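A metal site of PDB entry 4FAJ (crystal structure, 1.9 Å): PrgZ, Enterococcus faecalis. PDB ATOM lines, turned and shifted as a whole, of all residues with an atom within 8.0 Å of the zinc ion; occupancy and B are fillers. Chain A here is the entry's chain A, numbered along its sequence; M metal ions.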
ATOM      1  N   LYS A 278       2.697   4.231  21.088  1.00  0.00           N
ATOM      2  CA  LYS A 278       3.530   5.427  20.974  1.00  0.00           C
ATOM      3  C   LYS A 278       2.685   6.661  20.655  1.00  0.00           C
ATOM      4  O   LYS A 278       3.098   7.790  20.949  1.00  0.00           O
ATOM      5  CB  LYS A 278       4.557   5.240  19.865  1.00  0.00           C
ATOM      6  CG  LYS A 278       5.461   4.003  19.974  1.00  0.00           C
ATOM      7  CD  LYS A 278       6.914   4.349  20.346  1.00  0.00           C
ATOM      8  CE  LYS A 278       7.926   3.657  19.434  1.00  0.00           C
ATOM      9  NZ  LYS A 278       8.392   4.534  18.331  1.00  0.00           N
ATOM     10  N   GLU A 279       1.522   6.441  20.040  1.00  0.00           N
ATOM     11  CA  GLU A 279       0.612   7.522  19.648  1.00  0.00           C
ATOM     12  C   GLU A 279      -0.705   7.378  20.400  1.00  0.00           C
ATOM     13  O   GLU A 279      -1.434   6.408  20.220  1.00  0.00           O
ATOM     14  CB  GLU A 279       0.359   7.491  18.135  1.00  0.00           C
ATOM     15  CG  GLU A 279      -0.764   8.431  17.649  1.00  0.00           C
ATOM     16  CD  GLU A 279      -0.616   9.842  18.121  1.00  0.00           C
ATOM     17  OE1 GLU A 279       0.494  10.406  17.984  1.00  0.00           O
ATOM     18  OE2 GLU A 279      -1.597  10.427  18.651  1.00  0.00           O
ATOM     19  N   ILE A 280      -0.988   8.367  21.245  1.00  0.00           N
ATOM     20  CA  ILE A 280      -2.112   8.284  22.211  1.00  0.00           C
ATOM     21  C   ILE A 280      -3.482   8.217  21.527  1.00  0.00           C
ATOM     22  O   ILE A 280      -4.384   7.525  22.003  1.00  0.00           O
ATOM     23  CB  ILE A 280      -2.071   9.480  23.209  1.00  0.00           C
ATOM     24  CG1 ILE A 280      -0.728   9.515  23.963  1.00  0.00           C
ATOM     25  CG2 ILE A 280      -3.254   9.438  24.166  1.00  0.00           C
ATOM     26  CD1 ILE A 280      -0.278   8.200  24.551  1.00  0.00           C
ATOM     27  N   ASN A 281      -3.646   8.940  20.424  1.00  0.00           N
ATOM     28  CA  ASN A 281      -4.892   8.894  19.654  1.00  0.00           C
ATOM     29  C   ASN A 281      -5.241   7.474  19.229  1.00  0.00           C
ATOM     30  O   ASN A 281      -6.391   7.081  19.250  1.00  0.00           O
ATOM     31  CB  ASN A 281      -4.797   9.795  18.432  1.00  0.00           C
ATOM     32  CG  ASN A 281      -6.099   9.907  17.693  1.00  0.00           C
ATOM     33  OD1 ASN A 281      -7.052  10.482  18.191  1.00  0.00           O
ATOM     34  ND2 ASN A 281      -6.143   9.330  16.487  1.00  0.00           N
ATOM     35  N   THR A 282      -4.224   6.710  18.829  1.00  0.00           N
ATOM     36  CA  THR A 282      -4.438   5.344  18.368  1.00  0.00           C
ATOM     37  C   THR A 282      -4.822   4.433  19.540  1.00  0.00           C
ATOM     38  O   THR A 282      -5.710   3.617  19.404  1.00  0.00           O
ATOM     39  CB  THR A 282      -3.179   4.784  17.679  1.00  0.00           C
ATOM     40  OG1 THR A 282      -2.768   5.670  16.633  1.00  0.00           O
ATOM     41  CG2 THR A 282      -3.476   3.425  17.106  1.00  0.00           C
ATOM     42  N   ILE A 284      -6.391   5.246  22.267  1.00  0.00           N
ATOM     43  CA  ILE A 284      -7.736   5.594  22.670  1.00  0.00           C
ATOM     44  C   ILE A 284      -8.762   4.993  21.702  1.00  0.00           C
ATOM     45  O   ILE A 284      -9.762   4.402  22.128  1.00  0.00           O
ATOM     46  CB  ILE A 284      -7.905   7.125  22.744  1.00  0.00           C
ATOM     47  CG1 ILE A 284      -7.058   7.697  23.872  1.00  0.00           C
ATOM     48  CG2 ILE A 284      -9.362   7.499  22.890  1.00  0.00           C
ATOM     49  CD1 ILE A 284      -6.955   9.200  23.872  1.00  0.00           C
ATOM     50  N   ALA A 298      -2.280  11.619  28.129  1.00  0.00           N
ATOM     51  CA  ALA A 298      -1.563  12.844  28.470  1.00  0.00           C
ATOM     52  C   ALA A 298      -2.108  13.996  27.622  1.00  0.00           C
ATOM     53  O   ALA A 298      -2.851  13.769  26.682  1.00  0.00           O
ATOM     54  CB  ALA A 298      -0.083  12.678  28.208  1.00  0.00           C
ATOM     55  N   TYR A 301      -5.559  14.756  25.308  1.00  0.00           N
ATOM     56  CA  TYR A 301      -6.286  13.491  25.458  1.00  0.00           C
ATOM     57  C   TYR A 301      -6.690  13.283  26.920  1.00  0.00           C
ATOM     58  O   TYR A 301      -7.815  12.879  27.212  1.00  0.00           O
ATOM     59  CB  TYR A 301      -5.449  12.300  24.984  1.00  0.00           C
ATOM     60  CG  TYR A 301      -4.871  12.455  23.588  1.00  0.00           C
ATOM     61  CD1 TYR A 301      -5.671  12.264  22.457  1.00  0.00           C
ATOM     62  CD2 TYR A 301      -3.540  12.795  23.395  1.00  0.00           C
ATOM     63  CE1 TYR A 301      -5.158  12.394  21.164  1.00  0.00           C
ATOM     64  CE2 TYR A 301      -3.007  12.952  22.089  1.00  0.00           C
ATOM     65  CZ  TYR A 301      -3.825  12.741  20.989  1.00  0.00           C
ATOM     66  OH  TYR A 301      -3.316  12.863  19.711  1.00  0.00           O
ATOM     67  N   GLU A 421       5.118   9.780  21.247  1.00  0.00           N
ATOM     68  CA  GLU A 421       4.464  11.066  20.984  1.00  0.00           C
ATOM     69  C   GLU A 421       4.846  12.127  22.008  1.00  0.00           C
ATOM     70  O   GLU A 421       5.299  13.217  21.644  1.00  0.00           O
ATOM     71  CB  GLU A 421       2.932  10.921  20.963  1.00  0.00           C
ATOM     72  CG  GLU A 421       2.216  12.241  20.672  1.00  0.00           C
ATOM     73  CD  GLU A 421       0.714  12.106  20.611  1.00  0.00           C
ATOM     74  OE1 GLU A 421       0.187  11.038  20.965  1.00  0.00           O
ATOM     75  OE2 GLU A 421       0.059  13.087  20.154  1.00  0.00           O
ATOM     76  N   PHE A 422       4.644  11.822  23.281  1.00  0.00           N
ATOM     77  CA  PHE A 422       4.810  12.835  24.325  1.00  0.00           C
ATOM     78  C   PHE A 422       6.249  13.040  24.765  1.00  0.00           C
ATOM     79  O   PHE A 422       6.567  14.093  25.282  1.00  0.00           O
ATOM     80  CB  PHE A 422       3.853  12.582  25.489  1.00  0.00           C
ATOM     81  CG  PHE A 422       2.477  13.092  25.208  1.00  0.00           C
ATOM     82  CD1 PHE A 422       2.114  14.371  25.573  1.00  0.00           C
ATOM     83  CD2 PHE A 422       1.584  12.319  24.474  1.00  0.00           C
ATOM     84  CE1 PHE A 422       0.855  14.863  25.264  1.00  0.00           C
ATOM     85  CE2 PHE A 422       0.303  12.810  24.158  1.00  0.00           C
ATOM     86  CZ  PHE A 422      -0.045  14.091  24.542  1.00  0.00           C
ATOM     87  N   LYS A 425       7.234  15.567  22.168  1.00  0.00           N
ATOM     88  CA  LYS A 425       6.579  16.845  22.480  1.00  0.00           C
ATOM     89  C   LYS A 425       7.215  17.531  23.696  1.00  0.00           C
ATOM     90  O   LYS A 425       7.329  18.751  23.718  1.00  0.00           O
ATOM     91  CB  LYS A 425       5.095  16.624  22.741  1.00  0.00           C
ATOM     92  CG  LYS A 425       4.314  17.925  22.875  1.00  0.00           C
ATOM     93  CD  LYS A 425       2.917  17.657  23.392  1.00  0.00           C
ATOM     94  CE  LYS A 425       2.056  16.977  22.329  1.00  0.00           C
ATOM     95  NZ  LYS A 425       1.337  17.990  21.510  1.00  0.00           N
HETATM   96 ZN    ZN M   1      -1.485  12.358  19.098  1.00  0.00          ZN
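The side-chain carboxylate of Glu 421 sits at hydrogen-bond distance from the backbone NH of Ile 280 (2.9 Å).
The side-chain carboxylate (OE2) of Glu 279 sits close to the backbone NH (N) of Asn 281, 3.1 Å away.
The backbone NH of Glu 421 is in hydrogen-bond range of the backbone carbonyl oxygen of Lys 278 (2.9 Å).
Of the 11 residues printed, 3 come within 4 Å of the zinc ion.
The nearest printed residue that does not touch the zinc ion is Asn 281 (4.2 Å).
The zinc ion is bound by OE2 of Glu 279 (2.0 Å).
OH of Tyr 301 is bound to the zinc ion, 2.0 Å away.
The zinc ion is bound by the side-chain carboxylate (OE2) of Glu 421 (2.0 Å).
Slightly farther from the zinc ion lies the side-chain carboxylate (OE1) of Glu 421 (2.8 Å).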
